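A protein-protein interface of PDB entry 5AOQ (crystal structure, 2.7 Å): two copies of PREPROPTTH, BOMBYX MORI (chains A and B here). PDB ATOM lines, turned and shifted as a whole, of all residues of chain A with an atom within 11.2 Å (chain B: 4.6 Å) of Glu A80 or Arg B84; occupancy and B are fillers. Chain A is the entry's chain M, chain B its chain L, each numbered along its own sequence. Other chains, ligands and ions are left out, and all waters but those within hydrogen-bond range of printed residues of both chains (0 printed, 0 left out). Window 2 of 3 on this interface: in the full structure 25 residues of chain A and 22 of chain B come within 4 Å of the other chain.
OE2 of Glu A80 lies within salt-bridge range of NH2 of Arg B66 (3.8 Å). NE of Arg B84 is in salt-bridge range of OE1 of Glu A80, at 3.4 Å.
The backbone NH (N) of Arg B67 lies within hydrogen-bond range of the backbone carbonyl oxygen (O) of Arg B84 (3.1 Å).
Among the printed residues, pairs that only touch across the chains: Pro A78 with Trp B85, Leu A81 with Trp B85, Leu A81 with Lys B82, Trp A85 with Lys B82 and Glu A80 with Trp B85.
Of the printed residues of chain B, Pro A78 touches Trp B85 (3.4 Å). Printed residues of chain B within 4 Å of Leu A81: Lys B82 (3.5 Å) and Trp B85 (3.4 Å). Lys A82 touches none of the printed residues of chain B. Printed residues of chain B within 4 Å of Trp A85: Lys B82. Printed residues of chain A within 4 Å of Lys B82: Leu A81 (3.5 Å) and Trp A85 (3.8 Å). Of chain A, only Glu A80 (3.4 Å) comes within 4 Å of Arg B84. Of chain A, only Pro A78, Glu A80 and Leu A81 come within 4 Å of Trp B85. The nearest printed residue of chain B that does not touch Glu A80 is Lys B82 (6.9 Å). The nearest printed residue of chain B that does not touch Pro A78 is Arg B66 (5.4 Å).
Printed residues of chain A that touch a printed residue of chain B: Pro A78, Glu A80, Leu A81 and Trp A85. Hydrophobic or aromatic side chains of chain A within 4 Å of the printed part of chain B: Pro A78, Leu A81 and Trp A85. Of the 7 printed residues of chain B, 4 touch a printed residue of chain A. Hydrophobic or aromatic side chains of chain B within 4 Å of the printed part of chain A: Trp B85. Among the printed residues, 7 pairs touch across the chains. Among the printed residues, Asp or Glu carboxylates within 4 Å of a Lys or Arg side-chain nitrogen of the other chain: Glu A80 with Arg B66 (3.8 Å) and Glu A80 with Arg B84 (3.4 Å).
Trp A85 touches Lys B82, but with the chains exchanged Lys A82 does not touch Trp B85 (8.1 Å). Positions printed for both chains: 82, 83, 84, 85 and 86. Of the 7 pairs that touch across the chains among the printed residues, none has its exchanged pair printed and touching as well.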
ATOM      1  N   LEU A  64      -5.882 -19.966  33.533  1.00  0.00           N
ATOM      2  CA  LEU A  64      -6.991 -19.078  33.191  1.00  0.00           C
ATOM      3  C   LEU A  64      -8.193 -19.304  34.106  1.00  0.00           C
ATOM      4  O   LEU A  64      -8.542 -20.446  34.409  1.00  0.00           O
ATOM      5  CB  LEU A  64      -7.407 -19.284  31.732  1.00  0.00           C
ATOM      6  CG  LEU A  64      -6.346 -19.021  30.659  1.00  0.00           C
ATOM      7  CD1 LEU A  64      -6.914 -19.274  29.274  1.00  0.00           C
ATOM      8  CD2 LEU A  64      -5.805 -17.608  30.757  1.00  0.00           C
ATOM      9  N   LYS A  65      -8.819 -18.211  34.542  1.00  0.00           N
ATOM     10  CA  LYS A  65      -9.989 -18.277  35.421  1.00  0.00           C
ATOM     11  C   LYS A  65     -11.288 -18.063  34.638  1.00  0.00           C
ATOM     12  O   LYS A  65     -11.261 -17.603  33.497  1.00  0.00           O
ATOM     13  CB  LYS A  65      -9.872 -17.241  36.542  1.00  0.00           C
ATOM     14  CG  LYS A  65      -8.605 -17.372  37.383  1.00  0.00           C
ATOM     15  CD  LYS A  65      -8.604 -18.631  38.247  1.00  0.00           C
ATOM     16  CE  LYS A  65      -9.537 -18.496  39.443  1.00  0.00           C
ATOM     17  NZ  LYS A  65      -9.468 -19.681  40.345  1.00  0.00           N
ATOM     18  N   SER A  71     -13.007 -10.960  37.158  1.00  0.00           N
ATOM     19  CA  SER A  71     -11.917 -10.746  36.219  1.00  0.00           C
ATOM     20  C   SER A  71     -10.870  -9.803  36.801  1.00  0.00           C
ATOM     21  O   SER A  71     -10.780  -8.639  36.409  1.00  0.00           O
ATOM     22  CB  SER A  71     -12.443 -10.201  34.889  1.00  0.00           C
ATOM     23  OG  SER A  71     -13.278 -11.150  34.251  1.00  0.00           O
ATOM     24  N   SER A  74      -5.178  -9.487  35.031  1.00  0.00           N
ATOM     25  CA  SER A  74      -4.396 -10.433  34.247  1.00  0.00           C
ATOM     26  C   SER A  74      -3.023  -9.839  33.974  1.00  0.00           C
ATOM     27  O   SER A  74      -2.882  -8.621  33.868  1.00  0.00           O
ATOM     28  CB  SER A  74      -5.096 -10.763  32.928  1.00  0.00           C
ATOM     29  OG  SER A  74      -5.087  -9.640  32.064  1.00  0.00           O
ATOM     30  N   GLU A  76      -1.073 -10.481  31.160  1.00  0.00           N
ATOM     31  CA  GLU A  76      -1.141 -10.068  29.763  1.00  0.00           C
ATOM     32  C   GLU A  76      -1.854 -11.128  28.935  1.00  0.00           C
ATOM     33  O   GLU A  76      -1.327 -12.222  28.731  1.00  0.00           O
ATOM     34  CB  GLU A  76       0.260  -9.827  29.195  1.00  0.00           C
ATOM     35  CG  GLU A  76       0.271  -9.155  27.830  1.00  0.00           C
ATOM     36  CD  GLU A  76      -0.155  -7.699  27.882  1.00  0.00           C
ATOM     37  OE1 GLU A  76      -0.239  -7.136  28.995  1.00  0.00           O
ATOM     38  OE2 GLU A  76      -0.404  -7.116  26.807  1.00  0.00           O
ATOM     39  N   ILE A  77      -3.052 -10.799  28.464  1.00  0.00           N
ATOM     40  CA  ILE A  77      -3.819 -11.697  27.607  1.00  0.00           C
ATOM     41  C   ILE A  77      -4.521 -10.903  26.511  1.00  0.00           C
ATOM     42  O   ILE A  77      -4.832  -9.728  26.700  1.00  0.00           O
ATOM     43  CB  ILE A  77      -4.863 -12.498  28.408  1.00  0.00           C
ATOM     44  CG1 ILE A  77      -5.674 -11.559  29.306  1.00  0.00           C
ATOM     45  CG2 ILE A  77      -4.174 -13.563  29.243  1.00  0.00           C
ATOM     46  CD1 ILE A  77      -6.807 -12.235  30.056  1.00  0.00           C
ATOM     47  N   PRO A  78      -4.768 -11.543  25.356  1.00  0.00           N
ATOM     48  CA  PRO A  78      -5.448 -10.863  24.248  1.00  0.00           C
ATOM     49  C   PRO A  78      -6.840 -10.376  24.642  1.00  0.00           C
ATOM     50  O   PRO A  78      -7.540 -11.048  25.400  1.00  0.00           O
ATOM     51  CB  PRO A  78      -5.522 -11.940  23.158  1.00  0.00           C
ATOM     52  CG  PRO A  78      -5.301 -13.235  23.862  1.00  0.00           C
ATOM     53  CD  PRO A  78      -4.421 -12.934  25.022  1.00  0.00           C
ATOM     54  N   ASN A  79      -7.228  -9.214  24.127  1.00  0.00           N
ATOM     55  CA  ASN A  79      -8.469  -8.563  24.529  1.00  0.00           C
ATOM     56  C   ASN A  79      -9.722  -9.349  24.149  1.00  0.00           C
ATOM     57  O   ASN A  79     -10.826  -9.003  24.570  1.00  0.00           O
ATOM     58  CB  ASN A  79      -8.535  -7.160  23.927  1.00  0.00           C
ATOM     59  CG  ASN A  79      -7.499  -6.224  24.522  1.00  0.00           C
ATOM     60  OD1 ASN A  79      -6.565  -6.663  25.194  1.00  0.00           O
ATOM     61  ND2 ASN A  79      -7.659  -4.929  24.277  1.00  0.00           N
ATOM     62  N   GLU A  80      -9.555 -10.401  23.354  1.00  0.00           N
ATOM     63  CA  GLU A  80     -10.656 -11.317  23.079  1.00  0.00           C
ATOM     64  C   GLU A  80     -10.966 -12.157  24.315  1.00  0.00           C
ATOM     65  O   GLU A  80     -12.037 -12.757  24.410  1.00  0.00           O
ATOM     66  CB  GLU A  80     -10.329 -12.234  21.898  1.00  0.00           C
ATOM     67  CG  GLU A  80     -10.367 -11.550  20.539  1.00  0.00           C
ATOM     68  CD  GLU A  80     -10.199 -12.529  19.388  1.00  0.00           C
ATOM     69  OE1 GLU A  80     -10.186 -13.753  19.639  1.00  0.00           O
ATOM     70  OE2 GLU A  80     -10.080 -12.073  18.231  1.00  0.00           O
ATOM     71  N   LEU A  81     -10.025 -12.188  25.259  1.00  0.00           N
ATOM     72  CA  LEU A  81     -10.133 -13.044  26.438  1.00  0.00           C
ATOM     73  C   LEU A  81     -10.187 -12.256  27.746  1.00  0.00           C
ATOM     74  O   LEU A  81      -9.886 -12.794  28.811  1.00  0.00           O
ATOM     75  CB  LEU A  81      -8.959 -14.026  26.474  1.00  0.00           C
ATOM     76  CG  LEU A  81      -8.829 -14.940  25.253  1.00  0.00           C
ATOM     77  CD1 LEU A  81      -7.617 -15.847  25.392  1.00  0.00           C
ATOM     78  CD2 LEU A  81     -10.094 -15.764  25.054  1.00  0.00           C
ATOM     79  N   LYS A  82     -10.567 -10.985  27.665  1.00  0.00           N
ATOM     80  CA  LYS A  82     -10.869 -10.206  28.860  1.00  0.00           C
ATOM     81  C   LYS A  82     -12.318 -10.458  29.254  1.00  0.00           C
ATOM     82  O   LYS A  82     -13.010 -11.242  28.607  1.00  0.00           O
ATOM     83  CB  LYS A  82     -10.645  -8.712  28.620  1.00  0.00           C
ATOM     84  CG  LYS A  82      -9.202  -8.309  28.395  1.00  0.00           C
ATOM     85  CD  LYS A  82      -9.120  -6.845  27.990  1.00  0.00           C
ATOM     86  CE  LYS A  82      -7.868  -6.175  28.529  1.00  0.00           C
ATOM     87  NZ  LYS A  82      -7.861  -4.714  28.237  1.00  0.00           N
ATOM     88  N   TYR A  83     -12.769  -9.802  30.322  1.00  0.00           N
ATOM     89  CA  TYR A  83     -14.181  -9.799  30.718  1.00  0.00           C
ATOM     90  C   TYR A  83     -14.684 -11.154  31.233  1.00  0.00           C
ATOM     91  O   TYR A  83     -15.339 -11.214  32.275  1.00  0.00           O
ATOM     92  CB  TYR A  83     -15.053  -9.342  29.542  1.00  0.00           C
ATOM     93  CG  TYR A  83     -14.458  -8.196  28.751  1.00  0.00           C
ATOM     94  CD1 TYR A  83     -14.403  -6.914  29.283  1.00  0.00           C
ATOM     95  CD2 TYR A  83     -13.950  -8.397  27.474  1.00  0.00           C
ATOM     96  CE1 TYR A  83     -13.858  -5.866  28.566  1.00  0.00           C
ATOM     97  CE2 TYR A  83     -13.404  -7.355  26.749  1.00  0.00           C
ATOM     98  CZ  TYR A  83     -13.360  -6.092  27.299  1.00  0.00           C
ATOM     99  OH  TYR A  83     -12.817  -5.053  26.580  1.00  0.00           O
ATOM    100  N   ARG A  84     -14.365 -12.220  30.504  1.00  0.00           N
ATOM    101  CA  ARG A  84     -14.820 -13.569  30.828  1.00  0.00           C
ATOM    102  C   ARG A  84     -13.691 -14.411  31.423  1.00  0.00           C
ATOM    103  O   ARG A  84     -13.927 -15.273  32.271  1.00  0.00           O
ATOM    104  CB  ARG A  84     -15.375 -14.250  29.571  1.00  0.00           C
ATOM    105  CG  ARG A  84     -16.439 -13.437  28.836  1.00  0.00           C
ATOM    106  CD  ARG A  84     -16.353 -13.611  27.324  1.00  0.00           C
ATOM    107  NE  ARG A  84     -16.894 -14.891  26.873  1.00  0.00           N
ATOM    108  CZ  ARG A  84     -16.982 -15.257  25.597  1.00  0.00           C
ATOM    109  NH1 ARG A  84     -16.561 -14.445  24.637  1.00  0.00           N
ATOM    110  NH2 ARG A  84     -17.490 -16.440  25.280  1.00  0.00           N
ATOM    111  N   TRP A  85     -12.465 -14.150  30.970  1.00  0.00           N
ATOM    112  CA  TRP A  85     -11.287 -14.902  31.405  1.00  0.00           C
ATOM    113  C   TRP A  85     -10.187 -14.007  31.972  1.00  0.00           C
ATOM    114  O   TRP A  85     -10.103 -12.822  31.646  1.00  0.00           O
ATOM    115  CB  TRP A  85     -10.720 -15.714  30.236  1.00  0.00           C
ATOM    116  CG  TRP A  85     -11.672 -16.720  29.665  1.00  0.00           C
ATOM    117  CD1 TRP A  85     -12.640 -16.495  28.731  1.00  0.00           C
ATOM    118  CD2 TRP A  85     -11.738 -18.115  29.982  1.00  0.00           C
ATOM    119  NE1 TRP A  85     -13.307 -17.662  28.449  1.00  0.00           N
ATOM    120  CE2 TRP A  85     -12.774 -18.672  29.206  1.00  0.00           C
ATOM    121  CE3 TRP A  85     -11.024 -18.948  30.848  1.00  0.00           C
ATOM    122  CZ2 TRP A  85     -13.113 -20.022  29.270  1.00  0.00           C
ATOM    123  CZ3 TRP A  85     -11.362 -20.287  30.911  1.00  0.00           C
ATOM    124  CH2 TRP A  85     -12.396 -20.811  30.126  1.00  0.00           C
ATOM    125  N   VAL A  86      -9.350 -14.594  32.821  1.00  0.00           N
ATOM    126  CA  VAL A  86      -8.171 -13.924  33.365  1.00  0.00           C
ATOM    127  C   VAL A  86      -7.031 -14.905  33.583  1.00  0.00           C
ATOM    128  O   VAL A  86      -7.212 -15.961  34.190  1.00  0.00           O
ATOM    129  CB  VAL A  86      -8.472 -13.210  34.702  1.00  0.00           C
ATOM    130  CG1 VAL A  86      -7.187 -12.726  35.383  1.00  0.00           C
ATOM    131  CG2 VAL A  86      -9.421 -12.059  34.484  1.00  0.00           C
ATOM    132  N   ALA A  87      -5.854 -14.533  33.087  1.00  0.00           N
ATOM    133  CA  ALA A  87      -4.653 -15.341  33.245  1.00  0.00           C
ATOM    134  C   ALA A  87      -3.915 -14.936  34.512  1.00  0.00           C
ATOM    135  O   ALA A  87      -3.689 -13.751  34.757  1.00  0.00           O
ATOM    136  CB  ALA A  87      -3.749 -15.192  32.035  1.00  0.00           C
ATOM    137  N   ARG B  66      -4.152 -20.548  18.509  1.00  0.00           N
ATOM    138  CA  ARG B  66      -5.460 -20.182  17.965  1.00  0.00           C
ATOM    139  C   ARG B  66      -5.732 -20.662  16.535  1.00  0.00           C
ATOM    140  O   ARG B  66      -4.949 -21.420  15.960  1.00  0.00           O
ATOM    141  CB  ARG B  66      -5.635 -18.660  18.051  1.00  0.00           C
ATOM    142  CG  ARG B  66      -4.538 -17.842  17.402  1.00  0.00           C
ATOM    143  CD  ARG B  66      -4.813 -16.358  17.580  1.00  0.00           C
ATOM    144  NE  ARG B  66      -6.038 -15.951  16.894  1.00  0.00           N
ATOM    145  CZ  ARG B  66      -6.882 -15.019  17.330  1.00  0.00           C
ATOM    146  NH1 ARG B  66      -6.658 -14.372  18.467  1.00  0.00           N
ATOM    147  NH2 ARG B  66      -7.967 -14.734  16.622  1.00  0.00           N
ATOM    148  N   ARG B  67      -6.862 -20.202  15.998  1.00  0.00           N
ATOM    149  CA  ARG B  67      -7.486 -20.712  14.773  1.00  0.00           C
ATOM    150  C   ARG B  67      -6.540 -21.214  13.681  1.00  0.00           C
ATOM    151  O   ARG B  67      -5.675 -20.484  13.195  1.00  0.00           O
ATOM    152  CB  ARG B  67      -8.390 -19.619  14.189  1.00  0.00           C
ATOM    153  CG  ARG B  67      -9.067 -19.970  12.868  1.00  0.00           C
ATOM    154  CD  ARG B  67      -9.835 -21.279  12.946  1.00  0.00           C
ATOM    155  NE  ARG B  67     -10.510 -21.588  11.688  1.00  0.00           N
ATOM    156  CZ  ARG B  67     -10.819 -22.815  11.278  1.00  0.00           C
ATOM    157  NH1 ARG B  67     -10.509 -23.872  12.020  1.00  0.00           N
ATOM    158  NH2 ARG B  67     -11.438 -22.989  10.118  1.00  0.00           N
ATOM    159  N   LYS B  82     -14.353 -22.493  22.842  1.00  0.00           N
ATOM    160  CA  LYS B  82     -13.047 -22.418  22.201  1.00  0.00           C
ATOM    161  C   LYS B  82     -12.731 -23.514  21.193  1.00  0.00           C
ATOM    162  O   LYS B  82     -12.377 -24.635  21.556  1.00  0.00           O
ATOM    163  CB  LYS B  82     -11.956 -22.424  23.272  1.00  0.00           C
ATOM    164  CG  LYS B  82     -12.185 -21.422  24.383  1.00  0.00           C
ATOM    165  CD  LYS B  82     -10.875 -20.839  24.872  1.00  0.00           C
ATOM    166  CE  LYS B  82     -11.099 -19.854  26.002  1.00  0.00           C
ATOM    167  NZ  LYS B  82      -9.882 -19.046  26.274  1.00  0.00           N
ATOM    168  N   TYR B  83     -12.883 -23.174  19.919  1.00  0.00           N
ATOM    169  CA  TYR B  83     -11.987 -23.693  18.899  1.00  0.00           C
ATOM    170  C   TYR B  83     -11.345 -22.490  18.216  1.00  0.00           C
ATOM    171  O   TYR B  83     -10.427 -22.630  17.409  1.00  0.00           O
ATOM    172  CB  TYR B  83     -12.690 -24.587  17.881  1.00  0.00           C
ATOM    173  CG  TYR B  83     -11.687 -25.346  17.045  1.00  0.00           C
ATOM    174  CD1 TYR B  83     -10.774 -26.203  17.645  1.00  0.00           C
ATOM    175  CD2 TYR B  83     -11.628 -25.188  15.667  1.00  0.00           C
ATOM    176  CE1 TYR B  83      -9.842 -26.889  16.904  1.00  0.00           C
ATOM    177  CE2 TYR B  83     -10.695 -25.876  14.911  1.00  0.00           C
ATOM    178  CZ  TYR B  83      -9.805 -26.725  15.538  1.00  0.00           C
ATOM    179  OH  TYR B  83      -8.871 -27.416  14.807  1.00  0.00           O
ATOM    180  N   ARG B  84     -11.844 -21.304  18.557  1.00  0.00           N
ATOM    181  CA  ARG B  84     -11.173 -20.053  18.239  1.00  0.00           C
ATOM    182  C   ARG B  84      -9.746 -20.107  18.778  1.00  0.00           C
ATOM    183  O   ARG B  84      -8.838 -19.474  18.239  1.00  0.00           O
ATOM    184  CB  ARG B  84     -11.938 -18.873  18.845  1.00  0.00           C
ATOM    185  CG  ARG B  84     -11.834 -17.572  18.069  1.00  0.00           C
ATOM    186  CD  ARG B  84     -12.798 -16.535  18.629  1.00  0.00           C
ATOM    187  NE  ARG B  84     -12.728 -15.261  17.918  1.00  0.00           N
ATOM    188  CZ  ARG B  84     -13.460 -14.946  16.852  1.00  0.00           C
ATOM    189  NH1 ARG B  84     -14.333 -15.811  16.348  1.00  0.00           N
ATOM    190  NH2 ARG B  84     -13.317 -13.758  16.282  1.00  0.00           N
ATOM    191  N   TRP B  85      -9.570 -20.875  19.853  1.00  0.00           N
ATOM    192  CA  TRP B  85      -8.262 -21.117  20.448  1.00  0.00           C
ATOM    193  C   TRP B  85      -7.951 -22.614  20.437  1.00  0.00           C
ATOM    194  O   TRP B  85      -8.850 -23.436  20.269  1.00  0.00           O
ATOM    195  CB  TRP B  85      -8.215 -20.555  21.867  1.00  0.00           C
ATOM    196  CG  TRP B  85      -8.446 -19.075  21.892  1.00  0.00           C
ATOM    197  CD1 TRP B  85      -9.646 -18.435  21.999  1.00  0.00           C
ATOM    198  CD2 TRP B  85      -7.452 -18.048  21.786  1.00  0.00           C
ATOM    199  NE1 TRP B  85      -9.461 -17.075  21.973  1.00  0.00           N
ATOM    200  CE2 TRP B  85      -8.123 -16.810  21.844  1.00  0.00           C
ATOM    201  CE3 TRP B  85      -6.060 -18.054  21.654  1.00  0.00           C
ATOM    202  CZ2 TRP B  85      -7.450 -15.593  21.773  1.00  0.00           C
ATOM    203  CZ3 TRP B  85      -5.394 -16.845  21.583  1.00  0.00           C
ATOM    204  CH2 TRP B  85      -6.089 -15.632  21.642  1.00  0.00           C
ATOM    205  N   VAL B  86      -6.675 -22.956  20.606  1.00  0.00           N
ATOM    206  CA  VAL B  86      -6.218 -24.338  20.494  1.00  0.00           C
ATOM    207  C   VAL B  86      -5.181 -24.647  21.570  1.00  0.00           C
ATOM    208  O   VAL B  86      -4.204 -23.917  21.724  1.00  0.00           O
ATOM    209  CB  VAL B  86      -5.608 -24.611  19.098  1.00  0.00           C
ATOM    210  CG1 VAL B  86      -4.992 -26.004  19.031  1.00  0.00           C
ATOM    211  CG2 VAL B  86      -6.663 -24.448  18.015  1.00  0.00           C
